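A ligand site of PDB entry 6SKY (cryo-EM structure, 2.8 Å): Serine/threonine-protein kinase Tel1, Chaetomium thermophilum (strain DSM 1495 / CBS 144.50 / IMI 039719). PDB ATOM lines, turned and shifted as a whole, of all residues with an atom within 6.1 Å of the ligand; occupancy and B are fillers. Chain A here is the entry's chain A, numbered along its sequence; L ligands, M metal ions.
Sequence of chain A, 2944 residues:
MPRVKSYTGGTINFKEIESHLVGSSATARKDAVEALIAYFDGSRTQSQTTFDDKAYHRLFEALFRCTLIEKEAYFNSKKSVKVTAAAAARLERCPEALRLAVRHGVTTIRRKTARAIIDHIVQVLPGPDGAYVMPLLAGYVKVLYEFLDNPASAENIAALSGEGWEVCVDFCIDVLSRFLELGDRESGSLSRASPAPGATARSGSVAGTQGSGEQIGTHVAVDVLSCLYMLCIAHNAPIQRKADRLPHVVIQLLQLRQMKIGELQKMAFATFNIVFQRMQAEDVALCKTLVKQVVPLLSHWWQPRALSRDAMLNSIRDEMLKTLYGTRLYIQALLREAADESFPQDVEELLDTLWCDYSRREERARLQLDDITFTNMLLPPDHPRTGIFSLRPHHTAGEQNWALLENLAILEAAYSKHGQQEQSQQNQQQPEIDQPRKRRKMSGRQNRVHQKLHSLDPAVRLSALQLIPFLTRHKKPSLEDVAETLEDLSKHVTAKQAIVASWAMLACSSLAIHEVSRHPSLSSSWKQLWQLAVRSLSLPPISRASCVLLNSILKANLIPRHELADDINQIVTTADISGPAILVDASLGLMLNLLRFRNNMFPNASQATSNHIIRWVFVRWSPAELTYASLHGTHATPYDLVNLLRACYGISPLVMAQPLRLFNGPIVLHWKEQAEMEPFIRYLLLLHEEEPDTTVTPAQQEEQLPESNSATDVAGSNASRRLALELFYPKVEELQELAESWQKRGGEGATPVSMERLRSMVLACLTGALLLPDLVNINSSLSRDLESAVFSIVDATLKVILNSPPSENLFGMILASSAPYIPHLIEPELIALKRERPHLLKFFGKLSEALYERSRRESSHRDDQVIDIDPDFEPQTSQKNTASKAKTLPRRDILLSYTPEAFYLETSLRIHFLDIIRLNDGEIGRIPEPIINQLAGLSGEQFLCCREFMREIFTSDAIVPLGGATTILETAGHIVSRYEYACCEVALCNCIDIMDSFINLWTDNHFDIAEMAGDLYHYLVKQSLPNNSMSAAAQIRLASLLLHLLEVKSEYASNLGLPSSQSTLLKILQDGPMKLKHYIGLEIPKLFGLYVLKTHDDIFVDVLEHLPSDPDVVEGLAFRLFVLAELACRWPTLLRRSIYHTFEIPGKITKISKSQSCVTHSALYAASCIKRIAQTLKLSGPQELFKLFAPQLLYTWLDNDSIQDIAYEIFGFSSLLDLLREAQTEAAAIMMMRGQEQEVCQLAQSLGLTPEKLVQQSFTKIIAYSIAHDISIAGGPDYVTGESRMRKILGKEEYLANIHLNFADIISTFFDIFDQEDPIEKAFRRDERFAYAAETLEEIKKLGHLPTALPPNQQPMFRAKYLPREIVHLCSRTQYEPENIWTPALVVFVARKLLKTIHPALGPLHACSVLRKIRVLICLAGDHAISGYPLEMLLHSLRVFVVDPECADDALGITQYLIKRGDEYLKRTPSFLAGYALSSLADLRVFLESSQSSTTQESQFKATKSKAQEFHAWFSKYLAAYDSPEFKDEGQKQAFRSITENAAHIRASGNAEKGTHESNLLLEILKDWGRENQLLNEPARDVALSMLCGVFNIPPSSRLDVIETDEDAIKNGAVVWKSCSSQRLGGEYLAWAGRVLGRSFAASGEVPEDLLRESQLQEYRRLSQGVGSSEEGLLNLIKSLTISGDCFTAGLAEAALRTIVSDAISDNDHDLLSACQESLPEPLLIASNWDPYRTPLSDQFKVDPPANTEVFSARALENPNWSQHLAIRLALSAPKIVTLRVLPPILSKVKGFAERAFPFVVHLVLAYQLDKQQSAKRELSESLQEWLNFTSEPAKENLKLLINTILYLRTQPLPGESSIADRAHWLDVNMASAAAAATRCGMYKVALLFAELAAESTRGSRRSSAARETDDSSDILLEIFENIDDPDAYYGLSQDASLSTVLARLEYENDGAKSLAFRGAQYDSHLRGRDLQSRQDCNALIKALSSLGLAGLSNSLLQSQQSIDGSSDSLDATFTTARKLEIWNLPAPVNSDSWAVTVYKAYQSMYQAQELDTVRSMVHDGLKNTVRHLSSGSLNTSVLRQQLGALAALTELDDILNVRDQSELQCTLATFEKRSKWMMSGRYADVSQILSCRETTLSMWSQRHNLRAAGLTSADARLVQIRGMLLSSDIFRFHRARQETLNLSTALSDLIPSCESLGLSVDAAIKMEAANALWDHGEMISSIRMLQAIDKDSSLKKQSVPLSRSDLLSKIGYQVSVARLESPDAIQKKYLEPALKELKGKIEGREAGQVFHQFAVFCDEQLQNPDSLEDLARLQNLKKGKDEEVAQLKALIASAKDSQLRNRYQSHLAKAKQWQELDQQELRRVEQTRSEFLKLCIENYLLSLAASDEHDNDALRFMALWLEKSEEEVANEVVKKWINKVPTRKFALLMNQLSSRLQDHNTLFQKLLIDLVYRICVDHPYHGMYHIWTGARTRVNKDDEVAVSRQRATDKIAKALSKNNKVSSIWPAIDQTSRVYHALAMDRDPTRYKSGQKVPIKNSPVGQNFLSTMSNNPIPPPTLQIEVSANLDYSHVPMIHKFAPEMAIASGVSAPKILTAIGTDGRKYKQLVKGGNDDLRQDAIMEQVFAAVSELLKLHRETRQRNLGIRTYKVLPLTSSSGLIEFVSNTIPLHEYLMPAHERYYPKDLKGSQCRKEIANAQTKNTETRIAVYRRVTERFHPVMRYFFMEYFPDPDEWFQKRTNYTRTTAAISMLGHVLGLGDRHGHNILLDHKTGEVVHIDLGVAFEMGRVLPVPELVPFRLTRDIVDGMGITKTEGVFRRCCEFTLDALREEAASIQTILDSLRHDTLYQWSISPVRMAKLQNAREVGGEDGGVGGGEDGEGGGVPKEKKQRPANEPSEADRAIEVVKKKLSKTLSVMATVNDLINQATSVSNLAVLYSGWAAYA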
ATOM      1  N   ALA A2586      21.895 -15.661 -34.323  1.00  0.00           N
ATOM      2  CA  ALA A2586      22.172 -14.899 -33.118  1.00  0.00           C
ATOM      3  C   ALA A2586      23.035 -13.688 -33.438  1.00  0.00           C
ATOM      4  O   ALA A2586      23.562 -13.528 -34.541  1.00  0.00           O
ATOM      5  CB  ALA A2586      22.844 -15.792 -32.072  1.00  0.00           C
ATOM      6  N   SER A2587      23.195 -12.821 -32.441  1.00  0.00           N
ATOM      7  CA  SER A2587      23.886 -11.549 -32.625  1.00  0.00           C
ATOM      8  C   SER A2587      25.395 -11.735 -32.484  1.00  0.00           C
ATOM      9  O   SER A2587      25.877 -12.223 -31.459  1.00  0.00           O
ATOM     10  CB  SER A2587      23.383 -10.523 -31.614  1.00  0.00           C
ATOM     11  OG  SER A2587      21.987 -10.319 -31.758  1.00  0.00           O
ATOM     12  N   PRO A2592      26.324 -17.096 -35.473  1.00  0.00           N
ATOM     13  CA  PRO A2592      26.046 -18.473 -35.064  1.00  0.00           C
ATOM     14  C   PRO A2592      24.625 -18.833 -35.429  1.00  0.00           C
ATOM     15  O   PRO A2592      23.679 -18.158 -35.020  1.00  0.00           O
ATOM     16  CB  PRO A2592      26.263 -18.451 -33.542  1.00  0.00           C
ATOM     17  CG  PRO A2592      26.008 -17.056 -33.162  1.00  0.00           C
ATOM     18  CD  PRO A2592      26.404 -16.183 -34.323  1.00  0.00           C
ATOM     19  N   LEU A2608      23.689 -25.332 -32.289  1.00  0.00           N
ATOM     20  CA  LEU A2608      24.439 -24.151 -32.696  1.00  0.00           C
ATOM     21  C   LEU A2608      25.555 -24.621 -33.613  1.00  0.00           C
ATOM     22  O   LEU A2608      26.343 -25.495 -33.241  1.00  0.00           O
ATOM     23  CB  LEU A2608      25.030 -23.406 -31.513  1.00  0.00           C
ATOM     24  CG  LEU A2608      24.160 -22.690 -30.499  1.00  0.00           C
ATOM     25  CD1 LEU A2608      24.073 -23.506 -29.269  1.00  0.00           C
ATOM     26  CD2 LEU A2608      24.779 -21.359 -30.191  1.00  0.00           C
ATOM     27  N   LYS A2610      28.659 -23.210 -34.776  1.00  0.00           N
ATOM     28  CA  LYS A2610      29.467 -22.078 -34.352  1.00  0.00           C
ATOM     29  C   LYS A2610      30.705 -21.998 -35.228  1.00  0.00           C
ATOM     30  O   LYS A2610      31.465 -22.957 -35.331  1.00  0.00           O
ATOM     31  CB  LYS A2610      29.859 -22.211 -32.887  1.00  0.00           C
ATOM     32  CG  LYS A2610      29.703 -20.927 -32.106  1.00  0.00           C
ATOM     33  CD  LYS A2610      29.877 -21.200 -30.638  1.00  0.00           C
ATOM     34  CE  LYS A2610      29.442 -20.024 -29.805  1.00  0.00           C
ATOM     35  NZ  LYS A2610      29.518 -20.338 -28.346  1.00  0.00           N
ATOM     36  N   TYR A2649      25.947 -31.001 -21.389  1.00  0.00           N
ATOM     37  CA  TYR A2649      25.585 -30.832 -22.777  1.00  0.00           C
ATOM     38  C   TYR A2649      26.731 -31.387 -23.611  1.00  0.00           C
ATOM     39  O   TYR A2649      27.664 -31.975 -23.086  1.00  0.00           O
ATOM     40  CB  TYR A2649      25.220 -29.372 -23.096  1.00  0.00           C
ATOM     41  CG  TYR A2649      26.343 -28.371 -23.101  1.00  0.00           C
ATOM     42  CD1 TYR A2649      26.503 -27.522 -24.174  1.00  0.00           C
ATOM     43  CD2 TYR A2649      27.196 -28.223 -22.035  1.00  0.00           C
ATOM     44  CE1 TYR A2649      27.501 -26.594 -24.190  1.00  0.00           C
ATOM     45  CE2 TYR A2649      28.197 -27.303 -22.054  1.00  0.00           C
ATOM     46  CZ  TYR A2649      28.340 -26.491 -23.136  1.00  0.00           C
ATOM     47  OH  TYR A2649      29.343 -25.546 -23.170  1.00  0.00           O
ATOM     48  N   ILE A2661      27.464 -27.238 -31.151  1.00  0.00           N
ATOM     49  CA  ILE A2661      27.105 -27.236 -29.742  1.00  0.00           C
ATOM     50  C   ILE A2661      25.652 -27.645 -29.603  1.00  0.00           C
ATOM     51  O   ILE A2661      24.799 -27.219 -30.389  1.00  0.00           O
ATOM     52  CB  ILE A2661      27.351 -25.857 -29.110  1.00  0.00           C
ATOM     53  CG1 ILE A2661      28.778 -25.426 -29.384  1.00  0.00           C
ATOM     54  CG2 ILE A2661      27.155 -25.919 -27.649  1.00  0.00           C
ATOM     55  CD1 ILE A2661      29.136 -24.156 -28.720  1.00  0.00           C
ATOM     56  N   GLU A2662      25.381 -28.498 -28.634  1.00  0.00           N
ATOM     57  CA  GLU A2662      24.022 -28.942 -28.389  1.00  0.00           C
ATOM     58  C   GLU A2662      23.220 -27.808 -27.785  1.00  0.00           C
ATOM     59  O   GLU A2662      23.596 -27.264 -26.752  1.00  0.00           O
ATOM     60  CB  GLU A2662      24.029 -30.144 -27.459  1.00  0.00           C
ATOM     61  CG  GLU A2662      22.676 -30.688 -27.150  1.00  0.00           C
ATOM     62  CD  GLU A2662      22.692 -31.638 -25.983  1.00  0.00           C
ATOM     63  OE1 GLU A2662      22.425 -31.185 -24.851  1.00  0.00           O
ATOM     64  OE2 GLU A2662      22.986 -32.831 -26.187  1.00  0.00           O
ATOM     65  N   PHE A2663      22.123 -27.452 -28.435  1.00  0.00           N
ATOM     66  CA  PHE A2663      21.236 -26.415 -27.912  1.00  0.00           C
ATOM     67  C   PHE A2663      20.326 -27.066 -26.888  1.00  0.00           C
ATOM     68  O   PHE A2663      19.481 -27.893 -27.231  1.00  0.00           O
ATOM     69  CB  PHE A2663      20.447 -25.799 -29.056  1.00  0.00           C
ATOM     70  CG  PHE A2663      19.930 -24.430 -28.771  1.00  0.00           C
ATOM     71  CD1 PHE A2663      20.717 -23.331 -28.999  1.00  0.00           C
ATOM     72  CD2 PHE A2663      18.657 -24.253 -28.279  1.00  0.00           C
ATOM     73  CE1 PHE A2663      20.245 -22.072 -28.732  1.00  0.00           C
ATOM     74  CE2 PHE A2663      18.187 -23.003 -28.014  1.00  0.00           C
ATOM     75  CZ  PHE A2663      18.978 -21.913 -28.244  1.00  0.00           C
ATOM     76  N   VAL A2664      20.493 -26.702 -25.613  1.00  0.00           N
ATOM     77  CA  VAL A2664      19.781 -27.364 -24.528  1.00  0.00           C
ATOM     78  C   VAL A2664      18.297 -27.056 -24.645  1.00  0.00           C
ATOM     79  O   VAL A2664      17.897 -25.911 -24.868  1.00  0.00           O
ATOM     80  CB  VAL A2664      20.365 -26.963 -23.168  1.00  0.00           C
ATOM     81  CG1 VAL A2664      19.650 -27.673 -22.066  1.00  0.00           C
ATOM     82  CG2 VAL A2664      21.822 -27.298 -23.119  1.00  0.00           C
ATOM     83  N   THR A2667      15.284 -24.482 -22.135  1.00  0.00           N
ATOM     84  CA  THR A2667      15.831 -23.538 -21.183  1.00  0.00           C
ATOM     85  C   THR A2667      15.616 -22.109 -21.660  1.00  0.00           C
ATOM     86  O   THR A2667      15.059 -21.864 -22.728  1.00  0.00           O
ATOM     87  CB  THR A2667      17.321 -23.808 -20.984  1.00  0.00           C
ATOM     88  OG1 THR A2667      17.979 -23.687 -22.242  1.00  0.00           O
ATOM     89  CG2 THR A2667      17.547 -25.202 -20.453  1.00  0.00           C
ATOM     90  N   PRO A2669      18.085 -18.309 -21.156  1.00  0.00           N
ATOM     91  CA  PRO A2669      19.232 -17.716 -20.466  1.00  0.00           C
ATOM     92  C   PRO A2669      18.787 -16.881 -19.287  1.00  0.00           C
ATOM     93  O   PRO A2669      17.725 -16.270 -19.296  1.00  0.00           O
ATOM     94  CB  PRO A2669      19.890 -16.878 -21.554  1.00  0.00           C
ATOM     95  CG  PRO A2669      19.494 -17.535 -22.783  1.00  0.00           C
ATOM     96  CD  PRO A2669      18.116 -18.019 -22.585  1.00  0.00           C
ATOM     97  N   GLU A2672      18.211 -13.230 -20.150  1.00  0.00           N
ATOM     98  CA  GLU A2672      17.019 -13.000 -20.961  1.00  0.00           C
ATOM     99  C   GLU A2672      15.744 -13.121 -20.156  1.00  0.00           C
ATOM    100  O   GLU A2672      14.721 -12.557 -20.568  1.00  0.00           O
ATOM    101  CB  GLU A2672      16.967 -13.978 -22.117  1.00  0.00           C
ATOM    102  CG  GLU A2672      18.227 -14.064 -22.938  1.00  0.00           C
ATOM    103  CD  GLU A2672      18.371 -12.936 -23.934  1.00  0.00           C
ATOM    104  OE1 GLU A2672      18.306 -11.753 -23.530  1.00  0.00           O
ATOM    105  OE2 GLU A2672      18.550 -13.220 -25.132  1.00  0.00           O
ATOM    106  N   HIS A2762      28.854 -15.283 -16.048  1.00  0.00           N
ATOM    107  CA  HIS A2762      27.910 -14.198 -16.202  1.00  0.00           C
ATOM    108  C   HIS A2762      26.557 -14.749 -16.625  1.00  0.00           C
ATOM    109  O   HIS A2762      26.346 -15.960 -16.703  1.00  0.00           O
ATOM    110  CB  HIS A2762      28.436 -13.149 -17.181  1.00  0.00           C
ATOM    111  CG  HIS A2762      28.817 -13.689 -18.517  1.00  0.00           C
ATOM    112  ND1 HIS A2762      27.955 -13.711 -19.582  1.00  0.00           N
ATOM    113  CD2 HIS A2762      29.983 -14.218 -18.956  1.00  0.00           C
ATOM    114  CE1 HIS A2762      28.561 -14.240 -20.624  1.00  0.00           C
ATOM    115  NE2 HIS A2762      29.792 -14.557 -20.277  1.00  0.00           N
ATOM    116  N   GLY A2763      25.617 -13.863 -16.901  1.00  0.00           N
ATOM    117  CA  GLY A2763      24.248 -14.297 -17.099  1.00  0.00           C
ATOM    118  C   GLY A2763      23.953 -14.978 -18.408  1.00  0.00           C
ATOM    119  O   GLY A2763      22.859 -15.522 -18.565  1.00  0.00           O
ATOM    120  N   HIS A2764      24.879 -14.964 -19.363  1.00  0.00           N
ATOM    121  CA  HIS A2764      24.666 -15.613 -20.638  1.00  0.00           C
ATOM    122  C   HIS A2764      25.226 -17.010 -20.686  1.00  0.00           C
ATOM    123  O   HIS A2764      25.048 -17.698 -21.691  1.00  0.00           O
ATOM    124  CB  HIS A2764      25.272 -14.784 -21.761  1.00  0.00           C
ATOM    125  CG  HIS A2764      24.445 -13.606 -22.155  1.00  0.00           C
ATOM    126  ND1 HIS A2764      24.977 -12.370 -22.416  1.00  0.00           N
ATOM    127  CD2 HIS A2764      23.112 -13.489 -22.345  1.00  0.00           C
ATOM    128  CE1 HIS A2764      24.009 -11.536 -22.743  1.00  0.00           C
ATOM    129  NE2 HIS A2764      22.868 -12.184 -22.702  1.00  0.00           N
ATOM    130  N   ASN A2765      25.912 -17.445 -19.635  1.00  0.00           N
ATOM    131  CA  ASN A2765      26.439 -18.783 -19.518  1.00  0.00           C
ATOM    132  C   ASN A2765      25.621 -19.661 -18.595  1.00  0.00           C
ATOM    133  O   ASN A2765      25.988 -20.815 -18.383  1.00  0.00           O
ATOM    134  CB  ASN A2765      27.869 -18.735 -19.003  1.00  0.00           C
ATOM    135  CG  ASN A2765      28.859 -18.331 -20.054  1.00  0.00           C
ATOM    136  OD1 ASN A2765      28.625 -18.523 -21.232  1.00  0.00           O
ATOM    137  ND2 ASN A2765      29.960 -17.758 -19.634  1.00  0.00           N
ATOM    138  N   ILE A2766      24.530 -19.150 -18.061  1.00  0.00           N
ATOM    139  CA  ILE A2766      23.686 -19.858 -17.112  1.00  0.00           C
ATOM    140  C   ILE A2766      22.280 -19.904 -17.698  1.00  0.00           C
ATOM    141  O   ILE A2766      21.714 -18.859 -18.014  1.00  0.00           O
ATOM    142  CB  ILE A2766      23.691 -19.162 -15.736  1.00  0.00           C
ATOM    143  CG1 ILE A2766      25.117 -18.990 -15.250  1.00  0.00           C
ATOM    144  CG2 ILE A2766      22.880 -19.945 -14.746  1.00  0.00           C
ATOM    145  CD1 ILE A2766      25.236 -18.131 -14.038  1.00  0.00           C
ATOM    146  N   LEU A2767      21.750 -21.110 -17.852  1.00  0.00           N
ATOM    147  CA  LEU A2767      20.444 -21.338 -18.433  1.00  0.00           C
ATOM    148  C   LEU A2767      19.500 -21.868 -17.374  1.00  0.00           C
ATOM    149  O   LEU A2767      19.901 -22.669 -16.526  1.00  0.00           O
ATOM    150  CB  LEU A2767      20.532 -22.334 -19.586  1.00  0.00           C
ATOM    151  CG  LEU A2767      21.628 -22.135 -20.623  1.00  0.00           C
ATOM    152  CD1 LEU A2767      21.667 -23.321 -21.533  1.00  0.00           C
ATOM    153  CD2 LEU A2767      21.395 -20.892 -21.410  1.00  0.00           C
ATOM    154  N   ILE A2778      27.023 -23.564 -19.094  1.00  0.00           N
ATOM    155  CA  ILE A2778      27.641 -23.830 -20.377  1.00  0.00           C
ATOM    156  C   ILE A2778      28.903 -22.983 -20.448  1.00  0.00           C
ATOM    157  O   ILE A2778      29.173 -22.169 -19.574  1.00  0.00           O
ATOM    158  CB  ILE A2778      26.690 -23.525 -21.541  1.00  0.00           C
ATOM    159  CG1 ILE A2778      26.302 -22.057 -21.545  1.00  0.00           C
ATOM    160  CG2 ILE A2778      25.440 -24.338 -21.416  1.00  0.00           C
ATOM    161  CD1 ILE A2778      25.325 -21.708 -22.562  1.00  0.00           C
ATOM    162  N   ASP A2779      29.688 -23.188 -21.509  1.00  0.00           N
ATOM    163  CA  ASP A2779      30.848 -22.348 -21.793  1.00  0.00           C
ATOM    164  C   ASP A2779      31.867 -22.430 -20.657  1.00  0.00           C
ATOM    165  O   ASP A2779      32.236 -21.438 -20.040  1.00  0.00           O
ATOM    166  CB  ASP A2779      30.385 -20.912 -22.058  1.00  0.00           C
ATOM    167  CG  ASP A2779      31.438 -20.029 -22.695  1.00  0.00           C
ATOM    168  OD1 ASP A2779      32.587 -19.992 -22.222  1.00  0.00           O
ATOM    169  OD2 ASP A2779      31.081 -19.335 -23.676  1.00  0.00           O
ATOM    170  N   LYS A2859      38.495 -11.285 -26.222  1.00  0.00           N
ATOM    171  CA  LYS A2859      37.102 -11.596 -26.522  1.00  0.00           C
ATOM    172  C   LYS A2859      36.214 -11.620 -25.276  1.00  0.00           C
ATOM    173  O   LYS A2859      34.994 -11.669 -25.420  1.00  0.00           O
ATOM    174  CB  LYS A2859      37.022 -12.942 -27.238  1.00  0.00           C
ATOM    175  CG  LYS A2859      35.737 -13.174 -28.016  1.00  0.00           C
ATOM    176  CD  LYS A2859      35.829 -14.442 -28.863  1.00  0.00           C
ATOM    177  CE  LYS A2859      34.557 -14.650 -29.677  1.00  0.00           C
ATOM    178  NZ  LYS A2859      34.623 -15.889 -30.505  1.00  0.00           N
HETATM  179  P1  LIG L   1      28.942 -13.069 -25.660  1.00  0.00           P
HETATM  180  S1  LIG L   1      28.559 -12.439 -23.864  1.00  0.00           S
HETATM  181  O1  LIG L   1      29.894 -14.298 -25.620  1.00  0.00           O
HETATM  182  O2  LIG L   1      29.622 -11.937 -26.484  1.00  0.00           O
HETATM  183  P2  LIG L   1      26.939 -14.831 -26.012  1.00  0.00           P
HETATM  184  O3  LIG L   1      27.258 -15.218 -24.629  1.00  0.00           O
HETATM  185  O4  LIG L   1      25.452 -14.604 -26.302  1.00  0.00           O
HETATM  186  O5  LIG L   1      27.643 -13.486 -26.403  1.00  0.00           O
HETATM  187  P3  LIG L   1      26.414 -16.702 -27.950  1.00  0.00           P
HETATM  188  O6  LIG L   1      26.404 -16.060 -29.274  1.00  0.00           O
HETATM  189  O7  LIG L   1      26.799 -18.179 -27.956  1.00  0.00           O
HETATM  190  O8  LIG L   1      27.423 -15.983 -26.975  1.00  0.00           O
HETATM  191  O9  LIG L   1      24.984 -16.509 -27.333  1.00  0.00           O
HETATM  192  C1  LIG L   1      23.868 -17.122 -27.983  1.00  0.00           C
HETATM  193  C2  LIG L   1      22.671 -17.090 -27.070  1.00  0.00           C
HETATM  194  O10 LIG L   1      22.176 -18.436 -26.885  1.00  0.00           O
HETATM  195  C3  LIG L   1      22.924 -16.553 -25.667  1.00  0.00           C
HETATM  196  O11 LIG L   1      21.767 -15.920 -25.150  1.00  0.00           O
HETATM  197  C4  LIG L   1      23.291 -17.815 -24.884  1.00  0.00           C
HETATM  198  O12 LIG L   1      22.895 -17.695 -23.528  1.00  0.00           O
HETATM  199  C5  LIG L   1      22.459 -18.895 -25.573  1.00  0.00           C
HETATM  200  N1  LIG L   1      23.140 -20.174 -25.672  1.00  0.00           N
HETATM  201  C6  LIG L   1      24.468 -20.379 -25.912  1.00  0.00           C
HETATM  202  N2  LIG L   1      24.806 -21.637 -25.954  1.00  0.00           N
HETATM  203  C7  LIG L   1      23.624 -22.309 -25.725  1.00  0.00           C
HETATM  204  C8  LIG L   1      23.307 -23.679 -25.644  1.00  0.00           C
HETATM  205  N3  LIG L   1      24.213 -24.656 -25.787  1.00  0.00           N
HETATM  206  N4  LIG L   1      22.025 -24.010 -25.403  1.00  0.00           N
HETATM  207  C9  LIG L   1      21.125 -23.033 -25.253  1.00  0.00           C
HETATM  208  N5  LIG L   1      21.306 -21.715 -25.310  1.00  0.00           N
HETATM  209  C10 LIG L   1      22.583 -21.420 -25.546  1.00  0.00           C
HETATM  210 MG    MG M   1      28.684 -17.796 -24.121  1.00  0.00          MG
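An oxygen (O12) of the ligand sits at hydrogen-bond distance from the backbone carbonyl oxygen (O) of His 2764 (2.8 Å). N3 of the ligand lies within hydrogen-bond range of O of Glu 2662 (2.8 Å). A nitrogen (N4) of the ligand lies within hydrogen-bond range of the backbone NH (N) of Val 2664 (3.1 Å). NZ of Lys 2610 is in salt-bridge range of O7 of the ligand.
A ring nitrogen (ND1) of His 2762 lies close to the backbone NH (N) of His 2764 (3.3 Å). The side-chain hydroxyl (OG1) of Thr 2667 is in hydrogen-bond range of the backbone carbonyl oxygen (O) of Val 2664 (3.4 Å). The backbone carbonyl oxygen (O) of Asn 2765 sits at hydrogen-bond distance from the backbone NH (N) of Ile 2778 (3.0 Å). O of Ile 2661 sits at hydrogen-bond distance from N of Leu 2608. A ring nitrogen (NE2) of His 2762 lies within hydrogen-bond range of the side-chain amide nitrogen (ND2) of Asn 2765 (3.3 Å).
Leu 2608 touches the ligand. Ile 2661 touches the ligand (CG2 to N3, 3.7 Å). Phe 2663 touches the ligand. Pro 2669 touches the ligand (CG to O12, 3.5 Å). His 2762 touches the ligand. Leu 2767 touches the ligand. Ile 2778 touches the ligand. Within 4 Å of the ligand: Leu 2608, Lys 2610, Ile 2661, Glu 2662, Phe 2663, Val 2664, Pro 2669, His 2762, His 2764, Leu 2767 and Ile 2778. The nearest printed residue that does not touch the ligand is Tyr 2649 (4.01 Å).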
